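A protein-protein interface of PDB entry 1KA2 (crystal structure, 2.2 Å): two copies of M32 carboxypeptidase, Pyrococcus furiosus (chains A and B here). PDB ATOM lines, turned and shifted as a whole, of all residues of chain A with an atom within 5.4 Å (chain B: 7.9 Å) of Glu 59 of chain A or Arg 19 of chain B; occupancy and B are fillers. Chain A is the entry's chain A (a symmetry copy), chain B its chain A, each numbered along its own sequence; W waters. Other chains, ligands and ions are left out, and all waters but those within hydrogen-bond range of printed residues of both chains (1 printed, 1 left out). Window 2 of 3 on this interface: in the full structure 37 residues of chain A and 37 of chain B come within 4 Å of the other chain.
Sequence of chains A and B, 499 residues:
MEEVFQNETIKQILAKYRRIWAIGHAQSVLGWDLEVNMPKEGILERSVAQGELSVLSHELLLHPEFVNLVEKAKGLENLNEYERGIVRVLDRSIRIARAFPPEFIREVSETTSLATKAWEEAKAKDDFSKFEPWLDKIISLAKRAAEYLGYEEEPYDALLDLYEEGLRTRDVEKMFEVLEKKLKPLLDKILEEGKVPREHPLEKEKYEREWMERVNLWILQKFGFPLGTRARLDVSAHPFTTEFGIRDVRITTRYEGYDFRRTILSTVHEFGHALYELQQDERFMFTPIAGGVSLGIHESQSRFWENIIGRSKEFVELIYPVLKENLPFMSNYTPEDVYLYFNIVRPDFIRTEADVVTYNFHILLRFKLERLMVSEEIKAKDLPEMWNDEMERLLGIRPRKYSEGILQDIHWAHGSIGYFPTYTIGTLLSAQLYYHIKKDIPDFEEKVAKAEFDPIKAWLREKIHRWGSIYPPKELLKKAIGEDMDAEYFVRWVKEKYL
NH2 of Arg 19 of chain B is in salt-bridge range of OE1 of Glu 59 of chain A.
Of chain B, only Arg 19 (2.5 Å) comes within 4 Å of Glu 59 of chain A.
Of the printed residues of chain A, Arg 19 of chain B touches Glu 52 (3.2 Å), Val 55 (3.2 Å), Leu 56 (3.998 Å) and Glu 59 (2.5 Å).
Printed residues of chain A within 4 Å of Arg 18 of chain B: Glu 52 (3.5 Å).
Printed residues of chain B within 4 Å of Leu 56 of chain A: Arg 19 (3.998 Å), Ile 23 (3.9 Å) and Leu 56 (3.6 Å).
Of the printed residues of chain B, Val 55 of chain A touches Arg 19.
Of the printed residues of chain A, Ala 22 of chain B touches Glu 52 (3.4 Å).
Printed residues of chain A within 4 Å of Leu 56 of chain B: Leu 56 (3.6 Å).
The nearest printed residue of chain A that does not touch Arg 19 of chain B is Ser 57 of chain A (6.2 Å).
Leu 56 of chain A touches its own counterpart, Leu 56 of chain B.
Positions printed for both chains: 56, 57, 59, 60 and 63.
Of the 8 pairs that touch across the chains among the printed residues, 1 has its exchanged pair printed and touching as well.
Of the 20 printed residues of chain B, 5 touch a printed residue of chain A.
Printed residues of chain B that touch a printed residue of chain A: Arg 18, Arg 19, Ala 22, Ile 23 and Leu 56.
Hydrophobic or aromatic side chains of chain A within 4 Å of the printed part of chain B: Val 55 and Leu 56.
Among the printed residues, 8 pairs touch across the chains.
Among the printed residues, pairs that only touch across the chains: Glu 52 of chain A with Arg 18 of chain B, Glu 52 of chain A with Arg 19 of chain B, Glu 52 of chain A with Ala 22 of chain B, Val 55 of chain A with Arg 19 of chain B, Leu 56 of chain A with Arg 19 of chain B, Leu 56 of chain A with Ile 23 of chain B and Leu 56 of chain A with Leu 56 of chain B.
Water W1 lies within hydrogen-bond range of OE2 of Glu 52 of chain A (2.7 Å) and NH1 of Arg 18 of chain B (2.7 Å).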
ATOM      1  N   GLU A  52       2.959  -7.542  19.210  1.00  0.00           N
ATOM      2  CA  GLU A  52       3.272  -6.468  20.140  1.00  0.00           C
ATOM      3  C   GLU A  52       1.992  -5.903  20.764  1.00  0.00           C
ATOM      4  O   GLU A  52       1.952  -5.627  21.965  1.00  0.00           O
ATOM      5  CB  GLU A  52       4.038  -5.361  19.413  1.00  0.00           C
ATOM      6  CG  GLU A  52       5.445  -5.730  18.972  1.00  0.00           C
ATOM      7  CD  GLU A  52       6.393  -5.964  20.150  1.00  0.00           C
ATOM      8  OE1 GLU A  52       6.197  -5.357  21.220  1.00  0.00           O
ATOM      9  OE2 GLU A  52       7.347  -6.747  20.005  1.00  0.00           O
ATOM     10  N   SER A  54      -0.950  -7.464  21.144  1.00  0.00           N
ATOM     11  CA  SER A  54      -1.591  -8.420  22.050  1.00  0.00           C
ATOM     12  C   SER A  54      -0.949  -8.325  23.416  1.00  0.00           C
ATOM     13  O   SER A  54      -1.637  -8.384  24.435  1.00  0.00           O
ATOM     14  CB  SER A  54      -1.467  -9.855  21.537  1.00  0.00           C
ATOM     15  OG  SER A  54      -2.422 -10.101  20.522  1.00  0.00           O
ATOM     16  N   VAL A  55       0.371  -8.180  23.448  1.00  0.00           N
ATOM     17  CA  VAL A  55       1.042  -8.051  24.730  1.00  0.00           C
ATOM     18  C   VAL A  55       0.693  -6.702  25.364  1.00  0.00           C
ATOM     19  O   VAL A  55       0.538  -6.600  26.576  1.00  0.00           O
ATOM     20  CB  VAL A  55       2.578  -8.159  24.590  1.00  0.00           C
ATOM     21  CG1 VAL A  55       3.247  -7.798  25.912  1.00  0.00           C
ATOM     22  CG2 VAL A  55       2.965  -9.583  24.178  1.00  0.00           C
ATOM     23  N   LEU A  56       0.552  -5.672  24.538  1.00  0.00           N
ATOM     24  CA  LEU A  56       0.238  -4.350  25.055  1.00  0.00           C
ATOM     25  C   LEU A  56      -1.156  -4.377  25.652  1.00  0.00           C
ATOM     26  O   LEU A  56      -1.392  -3.878  26.757  1.00  0.00           O
ATOM     27  CB  LEU A  56       0.292  -3.309  23.930  1.00  0.00           C
ATOM     28  CG  LEU A  56       0.735  -1.884  24.287  1.00  0.00           C
ATOM     29  CD1 LEU A  56       0.389  -0.951  23.122  1.00  0.00           C
ATOM     30  CD2 LEU A  56       0.058  -1.416  25.568  1.00  0.00           C
ATOM     31  N   SER A  57      -2.075  -4.972  24.905  1.00  0.00           N
ATOM     32  CA  SER A  57      -3.465  -5.084  25.317  1.00  0.00           C
ATOM     33  C   SER A  57      -3.592  -5.769  26.684  1.00  0.00           C
ATOM     34  O   SER A  57      -4.226  -5.237  27.599  1.00  0.00           O
ATOM     35  CB  SER A  57      -4.239  -5.866  24.258  1.00  0.00           C
ATOM     36  OG  SER A  57      -5.622  -5.627  24.378  1.00  0.00           O
ATOM     37  N   HIS A  58      -2.984  -6.949  26.799  1.00  0.00           N
ATOM     38  CA  HIS A  58      -2.982  -7.754  28.022  1.00  0.00           C
ATOM     39  C   HIS A  58      -2.402  -6.945  29.180  1.00  0.00           C
ATOM     40  O   HIS A  58      -2.876  -7.023  30.312  1.00  0.00           O
ATOM     41  CB  HIS A  58      -2.132  -9.021  27.801  1.00  0.00           C
ATOM     42  CG  HIS A  58      -2.004  -9.902  29.011  1.00  0.00           C
ATOM     43  ND1 HIS A  58      -3.041 -10.681  29.483  1.00  0.00           N
ATOM     44  CD2 HIS A  58      -0.950 -10.151  29.825  1.00  0.00           C
ATOM     45  CE1 HIS A  58      -2.629 -11.374  30.530  1.00  0.00           C
ATOM     46  NE2 HIS A  58      -1.363 -11.071  30.759  1.00  0.00           N
ATOM     47  N   GLU A  59      -1.363  -6.174  28.881  1.00  0.00           N
ATOM     48  CA  GLU A  59      -0.712  -5.347  29.879  1.00  0.00           C
ATOM     49  C   GLU A  59      -1.670  -4.286  30.415  1.00  0.00           C
ATOM     50  O   GLU A  59      -1.733  -4.051  31.620  1.00  0.00           O
ATOM     51  CB  GLU A  59       0.520  -4.683  29.271  1.00  0.00           C
ATOM     52  CG  GLU A  59       1.353  -3.894  30.256  1.00  0.00           C
ATOM     53  CD  GLU A  59       2.602  -3.308  29.622  1.00  0.00           C
ATOM     54  OE1 GLU A  59       3.465  -4.094  29.156  1.00  0.00           O
ATOM     55  OE2 GLU A  59       2.714  -2.059  29.591  1.00  0.00           O
ATOM     56  N   LEU A  60      -2.421  -3.654  29.516  1.00  0.00           N
ATOM     57  CA  LEU A  60      -3.374  -2.614  29.904  1.00  0.00           C
ATOM     58  C   LEU A  60      -4.554  -3.178  30.701  1.00  0.00           C
ATOM     59  O   LEU A  60      -5.041  -2.554  31.647  1.00  0.00           O
ATOM     60  CB  LEU A  60      -3.899  -1.889  28.654  1.00  0.00           C
ATOM     61  CG  LEU A  60      -2.927  -1.014  27.851  1.00  0.00           C
ATOM     62  CD1 LEU A  60      -3.625  -0.454  26.616  1.00  0.00           C
ATOM     63  CD2 LEU A  60      -2.420   0.127  28.714  1.00  0.00           C
ATOM     64  N   LEU A  61      -5.024  -4.357  30.314  1.00  0.00           N
ATOM     65  CA  LEU A  61      -6.141  -4.975  31.004  1.00  0.00           C
ATOM     66  C   LEU A  61      -5.780  -5.334  32.441  1.00  0.00           C
ATOM     67  O   LEU A  61      -6.629  -5.294  33.331  1.00  0.00           O
ATOM     68  CB  LEU A  61      -6.583  -6.241  30.268  1.00  0.00           C
ATOM     69  CG  LEU A  61      -7.830  -6.941  30.815  1.00  0.00           C
ATOM     70  CD1 LEU A  61      -9.043  -6.026  30.624  1.00  0.00           C
ATOM     71  CD2 LEU A  61      -8.042  -8.263  30.090  1.00  0.00           C
ATOM     72  N   LEU A  62      -4.517  -5.678  32.671  1.00  0.00           N
ATOM     73  CA  LEU A  62      -4.088  -6.067  34.007  1.00  0.00           C
ATOM     74  C   LEU A  62      -3.328  -4.992  34.779  1.00  0.00           C
ATOM     75  O   LEU A  62      -2.693  -5.280  35.789  1.00  0.00           O
ATOM     76  CB  LEU A  62      -3.257  -7.354  33.929  1.00  0.00           C
ATOM     77  CG  LEU A  62      -4.013  -8.686  33.809  1.00  0.00           C
ATOM     78  CD1 LEU A  62      -5.080  -8.596  32.742  1.00  0.00           C
ATOM     79  CD2 LEU A  62      -3.024  -9.803  33.488  1.00  0.00           C
ATOM     80  N   HIS A  63      -3.394  -3.751  34.314  1.00  0.00           N
ATOM     81  CA  HIS A  63      -2.711  -2.673  35.017  1.00  0.00           C
ATOM     82  C   HIS A  63      -3.386  -2.511  36.385  1.00  0.00           C
ATOM     83  O   HIS A  63      -4.607  -2.578  36.489  1.00  0.00           O
ATOM     84  CB  HIS A  63      -2.820  -1.375  34.215  1.00  0.00           C
ATOM     85  CG  HIS A  63      -1.922  -0.287  34.710  1.00  0.00           C
ATOM     86  ND1 HIS A  63      -2.093   0.320  35.935  1.00  0.00           N
ATOM     87  CD2 HIS A  63      -0.821   0.276  34.159  1.00  0.00           C
ATOM     88  CE1 HIS A  63      -1.133   1.210  36.118  1.00  0.00           C
ATOM     89  NE2 HIS A  63      -0.349   1.202  35.056  1.00  0.00           N
ATOM     90  N   ILE B  13      16.699  -0.679  23.589  1.00  0.00           N
ATOM     91  CA  ILE B  13      15.897   0.369  22.988  1.00  0.00           C
ATOM     92  C   ILE B  13      15.041  -0.192  21.862  1.00  0.00           C
ATOM     93  O   ILE B  13      13.826   0.025  21.835  1.00  0.00           O
ATOM     94  CB  ILE B  13      16.796   1.501  22.442  1.00  0.00           C
ATOM     95  CG1 ILE B  13      17.406   2.279  23.610  1.00  0.00           C
ATOM     96  CG2 ILE B  13      15.993   2.418  21.524  1.00  0.00           C
ATOM     97  CD1 ILE B  13      18.410   3.343  23.189  1.00  0.00           C
ATOM     98  N   LEU B  14      15.669  -0.923  20.945  1.00  0.00           N
ATOM     99  CA  LEU B  14      14.954  -1.503  19.814  1.00  0.00           C
ATOM    100  C   LEU B  14      13.828  -2.439  20.243  1.00  0.00           C
ATOM    101  O   LEU B  14      12.797  -2.513  19.573  1.00  0.00           O
ATOM    102  CB  LEU B  14      15.925  -2.238  18.880  1.00  0.00           C
ATOM    103  CG  LEU B  14      16.979  -1.362  18.195  1.00  0.00           C
ATOM    104  CD1 LEU B  14      17.791  -2.198  17.208  1.00  0.00           C
ATOM    105  CD2 LEU B  14      16.303  -0.189  17.481  1.00  0.00           C
ATOM    106  N   ALA B  15      14.021  -3.147  21.353  1.00  0.00           N
ATOM    107  CA  ALA B  15      12.998  -4.055  21.869  1.00  0.00           C
ATOM    108  C   ALA B  15      11.779  -3.248  22.330  1.00  0.00           C
ATOM    109  O   ALA B  15      10.646  -3.628  22.065  1.00  0.00           O
ATOM    110  CB  ALA B  15      13.554  -4.873  23.031  1.00  0.00           C
ATOM    111  N   LYS B  16      12.009  -2.142  23.032  1.00  0.00           N
ATOM    112  CA  LYS B  16      10.894  -1.312  23.468  1.00  0.00           C
ATOM    113  C   LYS B  16      10.280  -0.611  22.264  1.00  0.00           C
ATOM    114  O   LYS B  16       9.070  -0.482  22.172  1.00  0.00           O
ATOM    115  CB  LYS B  16      11.351  -0.264  24.483  1.00  0.00           C
ATOM    116  CG  LYS B  16      11.739  -0.838  25.825  1.00  0.00           C
ATOM    117  CD  LYS B  16      12.300   0.238  26.746  1.00  0.00           C
ATOM    118  CE  LYS B  16      12.186  -0.189  28.193  1.00  0.00           C
ATOM    119  NZ  LYS B  16      10.758  -0.356  28.555  1.00  0.00           N
ATOM    120  N   TYR B  17      11.123  -0.164  21.337  1.00  0.00           N
ATOM    121  CA  TYR B  17      10.657   0.530  20.135  1.00  0.00           C
ATOM    122  C   TYR B  17       9.669  -0.299  19.293  1.00  0.00           C
ATOM    123  O   TYR B  17       8.781   0.262  18.616  1.00  0.00           O
ATOM    124  CB  TYR B  17      11.844   0.921  19.258  1.00  0.00           C
ATOM    125  CG  TYR B  17      11.442   1.795  18.097  1.00  0.00           C
ATOM    126  CD1 TYR B  17      11.075   3.120  18.308  1.00  0.00           C
ATOM    127  CD2 TYR B  17      11.377   1.285  16.800  1.00  0.00           C
ATOM    128  CE1 TYR B  17      10.647   3.927  17.259  1.00  0.00           C
ATOM    129  CE2 TYR B  17      10.943   2.082  15.734  1.00  0.00           C
ATOM    130  CZ  TYR B  17      10.580   3.406  15.981  1.00  0.00           C
ATOM    131  OH  TYR B  17      10.141   4.224  14.975  1.00  0.00           O
ATOM    132  N   ARG B  18       9.824  -1.622  19.330  1.00  0.00           N
ATOM    133  CA  ARG B  18       8.949  -2.516  18.574  1.00  0.00           C
ATOM    134  C   ARG B  18       7.474  -2.207  18.852  1.00  0.00           C
ATOM    135  O   ARG B  18       6.660  -2.174  17.934  1.00  0.00           O
ATOM    136  CB  ARG B  18       9.248  -3.984  18.919  1.00  0.00           C
ATOM    137  CG  ARG B  18      10.478  -4.562  18.240  1.00  0.00           C
ATOM    138  CD  ARG B  18      10.221  -5.990  17.824  1.00  0.00           C
ATOM    139  NE  ARG B  18      11.324  -6.501  17.021  1.00  0.00           N
ATOM    140  CZ  ARG B  18      11.367  -7.717  16.492  1.00  0.00           C
ATOM    141  NH1 ARG B  18      10.365  -8.560  16.678  1.00  0.00           N
ATOM    142  NH2 ARG B  18      12.409  -8.084  15.771  1.00  0.00           N
ATOM    143  N   ARG B  19       7.147  -1.990  20.125  1.00  0.00           N
ATOM    144  CA  ARG B  19       5.780  -1.672  20.539  1.00  0.00           C
ATOM    145  C   ARG B  19       5.333  -0.381  19.882  1.00  0.00           C
ATOM    146  O   ARG B  19       4.234  -0.276  19.360  1.00  0.00           O
ATOM    147  CB  ARG B  19       5.682  -1.482  22.058  1.00  0.00           C
ATOM    148  CG  ARG B  19       5.325  -2.706  22.827  1.00  0.00           C
ATOM    149  CD  ARG B  19       5.002  -2.373  24.259  1.00  0.00           C
ATOM    150  NE  ARG B  19       4.571  -3.577  24.963  1.00  0.00           N
ATOM    151  CZ  ARG B  19       4.216  -3.621  26.234  1.00  0.00           C
ATOM    152  NH1 ARG B  19       4.239  -2.524  26.962  1.00  0.00           N
ATOM    153  NH2 ARG B  19       3.827  -4.765  26.766  1.00  0.00           N
ATOM    154  N   ILE B  20       6.195   0.617  19.959  1.00  0.00           N
ATOM    155  CA  ILE B  20       5.896   1.901  19.367  1.00  0.00           C
ATOM    156  C   ILE B  20       5.731   1.663  17.870  1.00  0.00           C
ATOM    157  O   ILE B  20       4.784   2.156  17.255  1.00  0.00           O
ATOM    158  CB  ILE B  20       7.028   2.916  19.628  1.00  0.00           C
ATOM    159  CG1 ILE B  20       7.111   3.223  21.125  1.00  0.00           C
ATOM    160  CG2 ILE B  20       6.781   4.165  18.824  1.00  0.00           C
ATOM    161  CD1 ILE B  20       8.231   4.227  21.502  1.00  0.00           C
ATOM    162  N   TRP B  21       6.649   0.891  17.290  1.00  0.00           N
ATOM    163  CA  TRP B  21       6.579   0.591  15.868  1.00  0.00           C
ATOM    164  C   TRP B  21       5.263  -0.113  15.520  1.00  0.00           C
ATOM    165  O   TRP B  21       4.644   0.187  14.501  1.00  0.00           O
ATOM    166  CB  TRP B  21       7.762  -0.290  15.435  1.00  0.00           C
ATOM    167  CG  TRP B  21       7.654  -0.737  13.996  1.00  0.00           C
ATOM    168  CD1 TRP B  21       8.093  -0.068  12.888  1.00  0.00           C
ATOM    169  CD2 TRP B  21       6.976  -1.902  13.518  1.00  0.00           C
ATOM    170  NE1 TRP B  21       7.722  -0.741  11.746  1.00  0.00           N
ATOM    171  CE2 TRP B  21       7.033  -1.872  12.104  1.00  0.00           C
ATOM    172  CE3 TRP B  21       6.317  -2.970  14.149  1.00  0.00           C
ATOM    173  CZ2 TRP B  21       6.458  -2.873  11.304  1.00  0.00           C
ATOM    174  CZ3 TRP B  21       5.737  -3.972  13.350  1.00  0.00           C
ATOM    175  CH2 TRP B  21       5.813  -3.909  11.942  1.00  0.00           C
ATOM    176  N   ALA B  22       4.829  -1.043  16.363  1.00  0.00           N
ATOM    177  CA  ALA B  22       3.589  -1.771  16.105  1.00  0.00           C
ATOM    178  C   ALA B  22       2.351  -0.860  16.078  1.00  0.00           C
ATOM    179  O   ALA B  22       1.461  -1.030  15.238  1.00  0.00           O
ATOM    180  CB  ALA B  22       3.417  -2.874  17.145  1.00  0.00           C
ATOM    181  N   ILE B  23       2.276   0.089  17.007  1.00  0.00           N
ATOM    182  CA  ILE B  23       1.146   1.007  17.016  1.00  0.00           C
ATOM    183  C   ILE B  23       1.156   1.774  15.689  1.00  0.00           C
ATOM    184  O   ILE B  23       0.106   2.001  15.095  1.00  0.00           O
ATOM    185  CB  ILE B  23       1.231   1.993  18.210  1.00  0.00           C
ATOM    186  CG1 ILE B  23       1.102   1.216  19.521  1.00  0.00           C
ATOM    187  CG2 ILE B  23       0.119   3.036  18.129  1.00  0.00           C
ATOM    188  CD1 ILE B  23       1.229   2.092  20.750  1.00  0.00           C
ATOM    189  N   GLY B  24       2.347   2.147  15.214  1.00  0.00           N
ATOM    190  CA  GLY B  24       2.463   2.867  13.949  1.00  0.00           C
ATOM    191  C   GLY B  24       2.017   2.021  12.763  1.00  0.00           C
ATOM    192  O   GLY B  24       1.362   2.505  11.830  1.00  0.00           O
ATOM    193  N   HIS B  25       2.387   0.747  12.784  1.00  0.00           N
ATOM    194  CA  HIS B  25       1.977  -0.165  11.730  1.00  0.00           C
ATOM    195  C   HIS B  25       0.457  -0.107  11.722  1.00  0.00           C
ATOM    196  O   HIS B  25      -0.181   0.068  10.687  1.00  0.00           O
ATOM    197  CB  HIS B  25       2.416  -1.578  12.074  1.00  0.00           C
ATOM    198  CG  HIS B  25       1.943  -2.605  11.100  1.00  0.00           C
ATOM    199  ND1 HIS B  25       2.527  -2.783   9.865  1.00  0.00           N
ATOM    200  CD2 HIS B  25       0.940  -3.512  11.179  1.00  0.00           C
ATOM    201  CE1 HIS B  25       1.904  -3.758   9.224  1.00  0.00           C
ATOM    202  NE2 HIS B  25       0.938  -4.217  10.000  1.00  0.00           N
ATOM    203  N   ALA B  26      -0.116  -0.242  12.910  1.00  0.00           N
ATOM    204  CA  ALA B  26      -1.561  -0.209  13.066  1.00  0.00           C
ATOM    205  C   ALA B  26      -2.145   1.126  12.577  1.00  0.00           C
ATOM    206  O   ALA B  26      -3.136   1.134  11.865  1.00  0.00           O
ATOM    207  CB  ALA B  26      -1.926  -0.459  14.527  1.00  0.00           C
ATOM    208  N   LEU B  56      -1.546   6.855  23.083  1.00  0.00           N
ATOM    209  CA  LEU B  56      -0.820   5.727  23.642  1.00  0.00           C
ATOM    210  C   LEU B  56       0.612   5.771  23.142  1.00  0.00           C
ATOM    211  O   LEU B  56       1.566   5.610  23.908  1.00  0.00           O
ATOM    212  CB  LEU B  56      -1.470   4.405  23.214  1.00  0.00           C
ATOM    213  CG  LEU B  56      -1.402   3.221  24.186  1.00  0.00           C
ATOM    214  CD1 LEU B  56      -1.791   1.942  23.437  1.00  0.00           C
ATOM    215  CD2 LEU B  56      -0.006   3.091  24.780  1.00  0.00           C
ATOM    216  N   SER B  57       0.744   5.997  21.842  1.00  0.00           N
ATOM    217  CA  SER B  57       2.043   6.065  21.190  1.00  0.00           C
ATOM    218  C   SER B  57       2.946   7.116  21.847  1.00  0.00           C
ATOM    219  O   SER B  57       4.080   6.819  22.233  1.00  0.00           O
ATOM    220  CB  SER B  57       1.841   6.389  19.711  1.00  0.00           C
ATOM    221  OG  SER B  57       2.985   6.038  18.967  1.00  0.00           O
ATOM    222  N   GLU B  59       2.657   8.432  24.700  1.00  0.00           N
ATOM    223  CA  GLU B  59       2.916   8.033  26.071  1.00  0.00           C
ATOM    224  C   GLU B  59       4.108   7.082  26.145  1.00  0.00           C
ATOM    225  O   GLU B  59       4.966   7.221  27.013  1.00  0.00           O
ATOM    226  CB  GLU B  59       1.673   7.364  26.654  1.00  0.00           C
ATOM    227  CG  GLU B  59       1.782   7.018  28.121  1.00  0.00           C
ATOM    228  CD  GLU B  59       0.502   6.417  28.673  1.00  0.00           C
ATOM    229  OE1 GLU B  59      -0.541   7.119  28.670  1.00  0.00           O
ATOM    230  OE2 GLU B  59       0.545   5.241  29.106  1.00  0.00           O
ATOM    231  N   LEU B  60       4.160   6.122  25.225  1.00  0.00           N
ATOM    232  CA  LEU B  60       5.250   5.145  25.192  1.00  0.00           C
ATOM    233  C   LEU B  60       6.587   5.784  24.805  1.00  0.00           C
ATOM    234  O   LEU B  60       7.641   5.426  25.337  1.00  0.00           O
ATOM    235  CB  LEU B  60       4.915   4.017  24.203  1.00  0.00           C
ATOM    236  CG  LEU B  60       3.766   3.058  24.546  1.00  0.00           C
ATOM    237  CD1 LEU B  60       3.551   2.070  23.404  1.00  0.00           C
ATOM    238  CD2 LEU B  60       4.082   2.304  25.824  1.00  0.00           C
ATOM    239  N   HIS B  63       8.001   7.567  27.896  1.00  0.00           N
ATOM    240  CA  HIS B  63       8.073   6.843  29.158  1.00  0.00           C
ATOM    241  C   HIS B  63       9.489   7.030  29.719  1.00  0.00           C
ATOM    242  O   HIS B  63      10.464   6.981  28.976  1.00  0.00           O
ATOM    243  CB  HIS B  63       7.785   5.359  28.927  1.00  0.00           C
ATOM    244  CG  HIS B  63       7.562   4.588  30.188  1.00  0.00           C
ATOM    245  ND1 HIS B  63       8.559   4.369  31.114  1.00  0.00           N
ATOM    246  CD2 HIS B  63       6.443   4.017  30.694  1.00  0.00           C
ATOM    247  CE1 HIS B  63       8.063   3.697  32.138  1.00  0.00           C
ATOM    248  NE2 HIS B  63       6.781   3.472  31.908  1.00  0.00           N
ATOM    249  N   PHE B 286      11.687  -2.819  11.739  1.00  0.00           N
ATOM    250  CA  PHE B 286      11.220  -2.592  13.119  1.00  0.00           C
ATOM    251  C   PHE B 286      11.988  -1.504  13.890  1.00  0.00           C
ATOM    252  O   PHE B 286      11.706  -1.265  15.068  1.00  0.00           O
ATOM    253  CB  PHE B 286      11.290  -3.888  13.928  1.00  0.00           C
ATOM    254  CG  PHE B 286      10.704  -5.057  13.227  1.00  0.00           C
ATOM    255  CD1 PHE B 286      11.502  -6.134  12.869  1.00  0.00           C
ATOM    256  CD2 PHE B 286       9.354  -5.069  12.886  1.00  0.00           C
ATOM    257  CE1 PHE B 286      10.959  -7.222  12.174  1.00  0.00           C
ATOM    258  CE2 PHE B 286       8.806  -6.141  12.196  1.00  0.00           C
ATOM    259  CZ  PHE B 286       9.611  -7.223  11.838  1.00  0.00           C
HETATM  260  O   HOH W   1       8.312  -8.754  18.471  1.00  0.00           O
